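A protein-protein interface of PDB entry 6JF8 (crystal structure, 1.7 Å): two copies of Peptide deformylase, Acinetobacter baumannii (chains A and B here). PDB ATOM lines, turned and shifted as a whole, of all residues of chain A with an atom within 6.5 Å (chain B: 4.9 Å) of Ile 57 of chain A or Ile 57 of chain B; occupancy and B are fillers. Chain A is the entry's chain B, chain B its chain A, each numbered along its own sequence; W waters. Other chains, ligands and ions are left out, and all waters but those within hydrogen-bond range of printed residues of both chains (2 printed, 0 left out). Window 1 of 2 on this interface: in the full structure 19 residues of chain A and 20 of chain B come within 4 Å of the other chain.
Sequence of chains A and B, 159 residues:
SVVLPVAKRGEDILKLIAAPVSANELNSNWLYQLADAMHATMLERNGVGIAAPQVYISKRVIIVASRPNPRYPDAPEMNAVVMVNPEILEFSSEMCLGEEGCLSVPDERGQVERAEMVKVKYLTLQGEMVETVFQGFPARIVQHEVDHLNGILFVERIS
The backbone carbonyl oxygen (O) of Ala 52 of chain B is in hydrogen-bond range of the backbone NH (N) of Ile 57 of chain B (3.1 Å).
O of Ala 52 of chain A sits at hydrogen-bond distance from N of Ile 57 of chain A.
Trp 30 of chain A touches Leu 34 of chain B, but with the chains exchanged Leu 34 of chain A does not touch Trp 30 of chain B (4.3 Å).
Trp 30 of chain A touches Ile 57 of chain B, and with the chains exchanged Ile 57 of chain A touches Trp 30 of chain B.
Tyr 56 of chain A touches Ser 58 of chain B, and with the chains exchanged Ser 58 of chain A touches Tyr 56 of chain B.
Ile 57 of chain B touches its own counterpart, Ile 57 of chain A.
Positions printed for both chains: 30, 34, 52, 53, 55, 56, 57, 58 and 59.
The backbone carbonyl oxygen (O) of Tyr 56 of chain B sits at hydrogen-bond distance from the backbone NH (N) of Ser 58 of chain A, at 2.8 Å.
O of Tyr 56 of chain A lies within hydrogen-bond range of N of Ser 58 of chain B.
Of the 9 printed residues of chain B, 6 touch a printed residue of chain A.
Printed residues of chain B that touch a printed residue of chain A: Trp 30, Leu 34, Val 55, Tyr 56, Ile 57 and Ser 58.
Hydrophobic or aromatic side chains of chain B that line the printed part of chain A: Trp 30, Tyr 56 and Ile 57.
Of the 18 printed residues of chain A, 7 touch a printed residue of chain B.
Hydrophobic or aromatic side chains of chain A within 4 Å of the printed part of chain B: Leu 4, Ile 13, Trp 30, Tyr 56 and Ile 57.
Among the printed residues, 12 pairs touch across the chains.
Water W2 bridges the backbone carbonyl oxygen of Val 55 of chain B (2.7 Å) and the side-chain amino group of Lys 59 of chain A (2.9 Å).
Water W1 bridges the backbone carbonyl oxygen of Val 55 of chain A (2.8 Å) and the side-chain amino group of Lys 59 of chain B (2.8 Å).
Trp 30 of chain B touches Leu 4 of chain A (NE1 to CD2, 3.5 Å).
Ile 13 of chain A touches Ser 58 of chain B.
CZ3 of Trp 30 of chain A touches CZ3 of Trp 30 of chain B, 3.8 Å away.
Leu 34 of chain B touches Trp 30 of chain A (CA to CZ3, 3.9 Å).
CD1 of Ile 57 of chain B touches CH2 of Trp 30 of chain A, 3.9 Å away.
Tyr 56 of chain A touches Ile 57 of chain B (O to C, 3.8 Å).
Ile 57 of chain A touches Trp 30 of chain B.
Ile 57 of chain A touches Tyr 56 of chain B.
Ile 57 of chain A touches Ile 57 of chain B.
Lys 59 of chain A touches Val 55 of chain B (CE to O, 3.8 Å).
Ile 57 of chain A touches just these residues of chain B: Trp 30, Tyr 56 and Ile 57.
Of the printed residues of chain B, Ser 58 of chain A touches Tyr 56.
Printed residues of chain A within 4 Å of Leu 34 of chain B: Trp 30.
Ile 57 of chain B touches just these residues of chain A: Trp 30 (3.9 Å), Tyr 56 (3.8 Å) and Ile 57 (3.5 Å).
Of the printed residues of chain A, Ser 58 of chain B touches Ile 13 (3.9 Å) and Tyr 56 (2.9 Å).
The nearest printed residue of chain B that does not touch Ile 57 of chain A is Ser 58 of chain B (5.0 Å).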
ATOM      1  N   LEU A   4      25.903  29.131  -6.987  1.00  0.00           N
ATOM      2  CA  LEU A   4      25.432  28.828  -5.653  1.00  0.00           C
ATOM      3  C   LEU A   4      25.588  30.002  -4.694  1.00  0.00           C
ATOM      4  O   LEU A   4      26.560  30.720  -4.833  1.00  0.00           O
ATOM      5  CB  LEU A   4      26.220  27.613  -5.069  1.00  0.00           C
ATOM      6  CG  LEU A   4      26.011  26.326  -5.822  1.00  0.00           C
ATOM      7  CD1 LEU A   4      27.028  25.293  -5.313  1.00  0.00           C
ATOM      8  CD2 LEU A   4      24.544  25.872  -5.687  1.00  0.00           C
ATOM      9  N   ILE A  13      28.208  27.599   9.455  1.00  0.00           N
ATOM     10  CA  ILE A  13      28.694  26.570   8.467  1.00  0.00           C
ATOM     11  C   ILE A  13      30.191  26.800   8.162  1.00  0.00           C
ATOM     12  O   ILE A  13      30.930  25.864   7.866  1.00  0.00           O
ATOM     13  CB  ILE A  13      27.871  26.618   7.160  1.00  0.00           C
ATOM     14  CG1 ILE A  13      28.212  25.466   6.189  1.00  0.00           C
ATOM     15  CG2 ILE A  13      27.953  27.982   6.504  1.00  0.00           C
ATOM     16  CD1 ILE A  13      27.943  24.103   6.678  1.00  0.00           C
ATOM     17  N   ALA A  18      34.935  20.327   7.840  1.00  0.00           N
ATOM     18  CA  ALA A  18      34.241  19.646   6.747  1.00  0.00           C
ATOM     19  C   ALA A  18      34.531  18.163   6.718  1.00  0.00           C
ATOM     20  O   ALA A  18      35.605  17.739   7.093  1.00  0.00           O
ATOM     21  CB  ALA A  18      34.612  20.270   5.416  1.00  0.00           C
ATOM     22  N   TRP A  30      27.030  13.104  -9.109  1.00  0.00           N
ATOM     23  CA  TRP A  30      26.891  13.913  -8.016  1.00  0.00           C
ATOM     24  C   TRP A  30      28.187  14.776  -7.795  1.00  0.00           C
ATOM     25  O   TRP A  30      28.084  15.955  -7.609  1.00  0.00           O
ATOM     26  CB  TRP A  30      26.605  13.039  -6.775  1.00  0.00           C
ATOM     27  CG  TRP A  30      27.050  13.573  -5.544  1.00  0.00           C
ATOM     28  CD1 TRP A  30      28.102  13.103  -4.806  1.00  0.00           C
ATOM     29  CD2 TRP A  30      26.503  14.662  -4.838  1.00  0.00           C
ATOM     30  NE1 TRP A  30      28.245  13.860  -3.669  1.00  0.00           N
ATOM     31  CE2 TRP A  30      27.283  14.849  -3.688  1.00  0.00           C
ATOM     32  CE3 TRP A  30      25.430  15.565  -5.098  1.00  0.00           C
ATOM     33  CZ2 TRP A  30      27.030  15.859  -2.764  1.00  0.00           C
ATOM     34  CZ3 TRP A  30      25.179  16.548  -4.204  1.00  0.00           C
ATOM     35  CH2 TRP A  30      25.984  16.730  -3.047  1.00  0.00           C
ATOM     36  N   LEU A  34      28.684  18.855  -8.230  1.00  0.00           N
ATOM     37  CA  LEU A  34      29.166  19.688  -7.113  1.00  0.00           C
ATOM     38  C   LEU A  34      30.351  20.505  -7.589  1.00  0.00           C
ATOM     39  O   LEU A  34      30.397  21.739  -7.345  1.00  0.00           O
ATOM     40  CB  LEU A  34      29.519  18.879  -5.811  1.00  0.00           C
ATOM     41  CG  LEU A  34      30.391  19.578  -4.765  1.00  0.00           C
ATOM     42  CD1 LEU A  34      29.530  20.652  -4.173  1.00  0.00           C
ATOM     43  CD2 LEU A  34      30.896  18.802  -3.577  1.00  0.00           C
ATOM     44  N   MET A  38      30.560  24.560  -7.945  1.00  0.00           N
ATOM     45  CA  MET A  38      31.568  25.316  -7.270  1.00  0.00           C
ATOM     46  C   MET A  38      32.385  26.195  -8.260  1.00  0.00           C
ATOM     47  O   MET A  38      32.644  27.376  -7.936  1.00  0.00           O
ATOM     48  CB  MET A  38      32.540  24.393  -6.515  1.00  0.00           C
ATOM     49  CG  MET A  38      31.872  23.833  -5.264  1.00  0.00           C
ATOM     50  SD  MET A  38      32.864  22.572  -4.384  1.00  0.00           S
ATOM     51  CE  MET A  38      34.240  23.585  -3.926  1.00  0.00           C
ATOM     52  N   ALA A  51      36.068  26.897  -1.584  1.00  0.00           N
ATOM     53  CA  ALA A  51      35.947  25.646  -0.784  1.00  0.00           C
ATOM     54  C   ALA A  51      34.479  25.275  -0.595  1.00  0.00           C
ATOM     55  O   ALA A  51      33.636  26.156  -0.424  1.00  0.00           O
ATOM     56  CB  ALA A  51      36.600  25.826   0.573  1.00  0.00           C
ATOM     57  N   ALA A  52      34.175  23.988  -0.568  1.00  0.00           N
ATOM     58  CA  ALA A  52      32.777  23.607  -0.496  1.00  0.00           C
ATOM     59  C   ALA A  52      31.988  24.209   0.653  1.00  0.00           C
ATOM     60  O   ALA A  52      30.791  24.578   0.458  1.00  0.00           O
ATOM     61  CB  ALA A  52      32.581  22.106  -0.625  1.00  0.00           C
ATOM     62  N   PRO A  53      32.563  24.374   1.865  1.00  0.00           N
ATOM     63  CA  PRO A  53      31.783  24.968   2.970  1.00  0.00           C
ATOM     64  C   PRO A  53      31.259  26.389   2.676  1.00  0.00           C
ATOM     65  O   PRO A  53      30.220  26.801   3.172  1.00  0.00           O
ATOM     66  CB  PRO A  53      32.776  25.006   4.113  1.00  0.00           C
ATOM     67  CG  PRO A  53      33.643  23.835   3.849  1.00  0.00           C
ATOM     68  CD  PRO A  53      33.769  23.686   2.387  1.00  0.00           C
ATOM     69  N   GLN A  54      31.949  27.108   1.783  1.00  0.00           N
ATOM     70  CA  GLN A  54      31.492  28.398   1.397  1.00  0.00           C
ATOM     71  C   GLN A  54      30.170  28.360   0.664  1.00  0.00           C
ATOM     72  O   GLN A  54      29.535  29.445   0.535  1.00  0.00           O
ATOM     73  CB  GLN A  54      32.542  29.099   0.524  1.00  0.00           C
ATOM     74  CG  GLN A  54      33.826  29.369   1.313  1.00  0.00           C
ATOM     75  CD  GLN A  54      34.809  30.086   0.458  1.00  0.00           C
ATOM     76  OE1 GLN A  54      35.473  29.511  -0.398  1.00  0.00           O
ATOM     77  NE2 GLN A  54      34.764  31.428   0.536  1.00  0.00           N
ATOM     78  N   VAL A  55      29.891  27.243   0.044  1.00  0.00           N
ATOM     79  CA  VAL A  55      28.576  27.100  -0.668  1.00  0.00           C
ATOM     80  C   VAL A  55      27.582  26.160   0.092  1.00  0.00           C
ATOM     81  O   VAL A  55      26.671  25.550  -0.490  1.00  0.00           O
ATOM     82  CB  VAL A  55      28.709  26.818  -2.131  1.00  0.00           C
ATOM     83  CG1 VAL A  55      29.348  27.956  -2.900  1.00  0.00           C
ATOM     84  CG2 VAL A  55      29.422  25.491  -2.378  1.00  0.00           C
ATOM     85  N   TYR A  56      27.788  26.094   1.400  1.00  0.00           N
ATOM     86  CA  TYR A  56      26.968  25.348   2.353  1.00  0.00           C
ATOM     87  C   TYR A  56      27.087  23.842   2.205  1.00  0.00           C
ATOM     88  O   TYR A  56      26.201  23.101   2.676  1.00  0.00           O
ATOM     89  CB  TYR A  56      25.438  25.725   2.322  1.00  0.00           C
ATOM     90  CG  TYR A  56      25.186  27.159   2.647  1.00  0.00           C
ATOM     91  CD1 TYR A  56      25.198  28.148   1.639  1.00  0.00           C
ATOM     92  CD2 TYR A  56      24.990  27.556   3.959  1.00  0.00           C
ATOM     93  CE1 TYR A  56      24.980  29.465   1.949  1.00  0.00           C
ATOM     94  CE2 TYR A  56      24.767  28.892   4.278  1.00  0.00           C
ATOM     95  CZ  TYR A  56      24.758  29.825   3.247  1.00  0.00           C
ATOM     96  OH  TYR A  56      24.549  31.172   3.551  1.00  0.00           O
ATOM     97  N   ILE A  57      28.204  23.367   1.692  1.00  0.00           N
ATOM     98  CA  ILE A  57      28.442  21.965   1.459  1.00  0.00           C
ATOM     99  C   ILE A  57      29.615  21.608   2.385  1.00  0.00           C
ATOM    100  O   ILE A  57      30.751  21.950   2.085  1.00  0.00           O
ATOM    101  CB  ILE A  57      28.705  21.645   0.025  1.00  0.00           C
ATOM    102  CG1 ILE A  57      27.482  22.063  -0.826  1.00  0.00           C
ATOM    103  CG2 ILE A  57      29.080  20.142  -0.121  1.00  0.00           C
ATOM    104  CD1 ILE A  57      27.753  21.886  -2.231  1.00  0.00           C
ATOM    105  N   SER A  58      29.340  20.907   3.483  1.00  0.00           N
ATOM    106  CA  SER A  58      30.395  20.697   4.519  1.00  0.00           C
ATOM    107  C   SER A  58      31.225  19.433   4.162  1.00  0.00           C
ATOM    108  O   SER A  58      31.220  18.434   4.864  1.00  0.00           O
ATOM    109  CB  SER A  58      29.786  20.625   5.879  1.00  0.00           C
ATOM    110  OG  SER A  58      30.777  20.815   6.855  1.00  0.00           O
ATOM    111  N   LYS A  59      31.889  19.497   3.003  1.00  0.00           N
ATOM    112  CA  LYS A  59      32.667  18.400   2.451  1.00  0.00           C
ATOM    113  C   LYS A  59      34.035  18.881   2.050  1.00  0.00           C
ATOM    114  O   LYS A  59      34.200  20.075   1.699  1.00  0.00           O
ATOM    115  CB  LYS A  59      31.997  17.785   1.303  1.00  0.00           C
ATOM    116  CG  LYS A  59      30.714  17.064   1.697  1.00  0.00           C
ATOM    117  CD  LYS A  59      30.156  16.356   0.484  1.00  0.00           C
ATOM    118  CE  LYS A  59      29.243  15.175   0.890  1.00  0.00           C
ATOM    119  NZ  LYS A  59      29.943  13.982   1.455  1.00  0.00           N
ATOM    120  N   ARG A  60      35.035  17.992   2.046  1.00  0.00           N
ATOM    121  CA  ARG A  60      36.393  18.403   1.771  1.00  0.00           C
ATOM    122  C   ARG A  60      36.740  18.421   0.321  1.00  0.00           C
ATOM    123  O   ARG A  60      37.414  17.531  -0.217  1.00  0.00           O
ATOM    124  CB  ARG A  60      37.390  17.530   2.587  1.00  0.00           C
ATOM    125  CG  ARG A  60      37.112  17.671   4.050  1.00  0.00           C
ATOM    126  CD  ARG A  60      38.040  16.861   5.004  1.00  0.00           C
ATOM    127  NE  ARG A  60      39.273  17.618   5.291  1.00  0.00           N
ATOM    128  CZ  ARG A  60      39.345  18.614   6.174  1.00  0.00           C
ATOM    129  NH1 ARG A  60      38.286  19.012   6.867  1.00  0.00           N
ATOM    130  NH2 ARG A  60      40.528  19.245   6.300  1.00  0.00           N
ATOM    131  N   VAL A  61      36.269  19.471  -0.369  1.00  0.00           N
ATOM    132  CA  VAL A  61      36.533  19.681  -1.754  1.00  0.00           C
ATOM    133  C   VAL A  61      36.909  21.156  -1.909  1.00  0.00           C
ATOM    134  O   VAL A  61      36.211  22.054  -1.337  1.00  0.00           O
ATOM    135  CB  VAL A  61      35.273  19.443  -2.622  1.00  0.00           C
ATOM    136  CG1 VAL A  61      35.541  19.669  -4.122  1.00  0.00           C
ATOM    137  CG2 VAL A  61      34.743  18.014  -2.533  1.00  0.00           C
ATOM    138  N   LEU A 149      38.174  24.409   5.103  1.00  0.00           N
ATOM    139  CA  LEU A 149      37.783  23.031   5.455  1.00  0.00           C
ATOM    140  C   LEU A 149      37.910  22.736   6.916  1.00  0.00           C
ATOM    141  O   LEU A 149      37.275  21.816   7.456  1.00  0.00           O
ATOM    142  CB  LEU A 149      38.529  22.010   4.647  1.00  0.00           C
ATOM    143  CG  LEU A 149      38.556  22.083   3.110  1.00  0.00           C
ATOM    144  CD1 LEU A 149      39.244  20.895   2.548  1.00  0.00           C
ATOM    145  CD2 LEU A 149      37.116  22.167   2.539  1.00  0.00           C
ATOM    146  N   TRP B  30      22.046  20.452 -10.632  1.00  0.00           N
ATOM    147  CA  TRP B  30      22.583  20.416  -9.274  1.00  0.00           C
ATOM    148  C   TRP B  30      21.533  19.927  -8.269  1.00  0.00           C
ATOM    149  O   TRP B  30      21.755  18.967  -7.519  1.00  0.00           O
ATOM    150  CB  TRP B  30      23.123  21.860  -8.904  1.00  0.00           C
ATOM    151  CG  TRP B  30      23.089  22.194  -7.446  1.00  0.00           C
ATOM    152  CD1 TRP B  30      22.287  23.101  -6.867  1.00  0.00           C
ATOM    153  CD2 TRP B  30      23.860  21.616  -6.412  1.00  0.00           C
ATOM    154  NE1 TRP B  30      22.447  23.111  -5.501  1.00  0.00           N
ATOM    155  CE2 TRP B  30      23.424  22.210  -5.193  1.00  0.00           C
ATOM    156  CE3 TRP B  30      24.842  20.618  -6.380  1.00  0.00           C
ATOM    157  CZ2 TRP B  30      23.957  21.878  -3.959  1.00  0.00           C
ATOM    158  CZ3 TRP B  30      25.359  20.234  -5.145  1.00  0.00           C
ATOM    159  CH2 TRP B  30      24.900  20.861  -3.933  1.00  0.00           C
ATOM    160  N   LEU B  34      21.328  16.329  -6.233  1.00  0.00           N
ATOM    161  CA  LEU B  34      21.281  16.299  -4.730  1.00  0.00           C
ATOM    162  C   LEU B  34      20.136  15.423  -4.236  1.00  0.00           C
ATOM    163  O   LEU B  34      20.324  14.502  -3.398  1.00  0.00           O
ATOM    164  CB  LEU B  34      21.152  17.751  -4.185  1.00  0.00           C
ATOM    165  CG  LEU B  34      20.755  17.777  -2.672  1.00  0.00           C
ATOM    166  CD1 LEU B  34      21.840  17.186  -1.823  1.00  0.00           C
ATOM    167  CD2 LEU B  34      20.563  19.164  -2.278  1.00  0.00           C
ATOM    168  N   ALA B  52      18.748  17.112   4.034  1.00  0.00           N
ATOM    169  CA  ALA B  52      20.083  17.378   3.425  1.00  0.00           C
ATOM    170  C   ALA B  52      21.250  17.564   4.464  1.00  0.00           C
ATOM    171  O   ALA B  52      22.301  17.038   4.199  1.00  0.00           O
ATOM    172  CB  ALA B  52      20.043  18.525   2.465  1.00  0.00           C
ATOM    173  N   PRO B  53      20.939  18.123   5.616  1.00  0.00           N
ATOM    174  CA  PRO B  53      22.026  18.295   6.613  1.00  0.00           C
ATOM    175  C   PRO B  53      22.587  16.924   7.081  1.00  0.00           C
ATOM    176  O   PRO B  53      23.749  16.851   7.454  1.00  0.00           O
ATOM    177  CB  PRO B  53      21.351  19.000   7.768  1.00  0.00           C
ATOM    178  CG  PRO B  53      20.352  19.881   7.060  1.00  0.00           C
ATOM    179  CD  PRO B  53      19.788  18.961   6.001  1.00  0.00           C
ATOM    180  N   VAL B  55      23.403  14.514   5.253  1.00  0.00           N
ATOM    181  CA  VAL B  55      24.400  14.155   4.269  1.00  0.00           C
ATOM    182  C   VAL B  55      25.398  15.334   4.053  1.00  0.00           C
ATOM    183  O   VAL B  55      26.064  15.397   3.048  1.00  0.00           O
ATOM    184  CB  VAL B  55      23.826  13.577   2.953  1.00  0.00           C
ATOM    185  CG1 VAL B  55      23.185  12.242   3.257  1.00  0.00           C
ATOM    186  CG2 VAL B  55      22.902  14.552   2.247  1.00  0.00           C
ATOM    187  N   TYR B  56      25.474  16.201   5.032  1.00  0.00           N
ATOM    188  CA  TYR B  56      26.477  17.285   5.175  1.00  0.00           C
ATOM    189  C   TYR B  56      26.163  18.480   4.226  1.00  0.00           C
ATOM    190  O   TYR B  56      27.061  19.259   3.871  1.00  0.00           O
ATOM    191  CB  TYR B  56      27.908  16.779   4.970  1.00  0.00           C
ATOM    192  CG  TYR B  56      28.405  15.792   6.049  1.00  0.00           C
ATOM    193  CD1 TYR B  56      28.886  16.271   7.237  1.00  0.00           C
ATOM    194  CD2 TYR B  56      28.321  14.425   5.863  1.00  0.00           C
ATOM    195  CE1 TYR B  56      29.332  15.415   8.240  1.00  0.00           C
ATOM    196  CE2 TYR B  56      28.707  13.529   6.868  1.00  0.00           C
ATOM    197  CZ  TYR B  56      29.235  14.052   8.015  1.00  0.00           C
ATOM    198  OH  TYR B  56      29.627  13.119   8.938  1.00  0.00           O
ATOM    199  N   ILE B  57      24.908  18.590   3.767  1.00  0.00           N
ATOM    200  CA  ILE B  57      24.514  19.646   2.793  1.00  0.00           C
ATOM    201  C   ILE B  57      23.572  20.549   3.551  1.00  0.00           C
ATOM    202  O   ILE B  57      22.480  20.118   3.941  1.00  0.00           O
ATOM    203  CB  ILE B  57      23.807  19.017   1.580  1.00  0.00           C
ATOM    204  CG1 ILE B  57      24.720  18.037   0.788  1.00  0.00           C
ATOM    205  CG2 ILE B  57      23.306  20.158   0.690  1.00  0.00           C
ATOM    206  CD1 ILE B  57      26.046  18.555   0.448  1.00  0.00           C
ATOM    207  N   SER B  58      24.025  21.757   3.960  1.00  0.00           N
ATOM    208  CA  SER B  58      23.264  22.590   4.866  1.00  0.00           C
ATOM    209  C   SER B  58      22.234  23.416   4.081  1.00  0.00           C
ATOM    210  O   SER B  58      22.323  24.641   4.017  1.00  0.00           O
ATOM    211  CB  SER B  58      24.209  23.462   5.703  1.00  0.00           C
ATOM    212  OG  SER B  58      23.494  23.984   6.835  1.00  0.00           O
ATOM    213  N   LYS B  59      21.319  22.706   3.350  1.00  0.00           N
ATOM    214  CA  LYS B  59      20.303  23.329   2.565  1.00  0.00           C
ATOM    215  C   LYS B  59      18.943  22.732   2.903  1.00  0.00           C
ATOM    216  O   LYS B  59      18.810  21.584   3.372  1.00  0.00           O
ATOM    217  CB  LYS B  59      20.545  22.996   1.071  1.00  0.00           C
ATOM    218  CG  LYS B  59      21.815  23.562   0.468  1.00  0.00           C
ATOM    219  CD  LYS B  59      21.529  24.920  -0.180  1.00  0.00           C
ATOM    220  CE  LYS B  59      22.610  25.334  -1.121  1.00  0.00           C
ATOM    221  NZ  LYS B  59      22.315  26.779  -1.339  1.00  0.00           N
HETATM  222  O   HOH W   1      25.004  27.300  -1.842  1.00  0.00           O
HETATM  223  O   HOH W   2      27.421  13.081   2.521  1.00  0.00           O
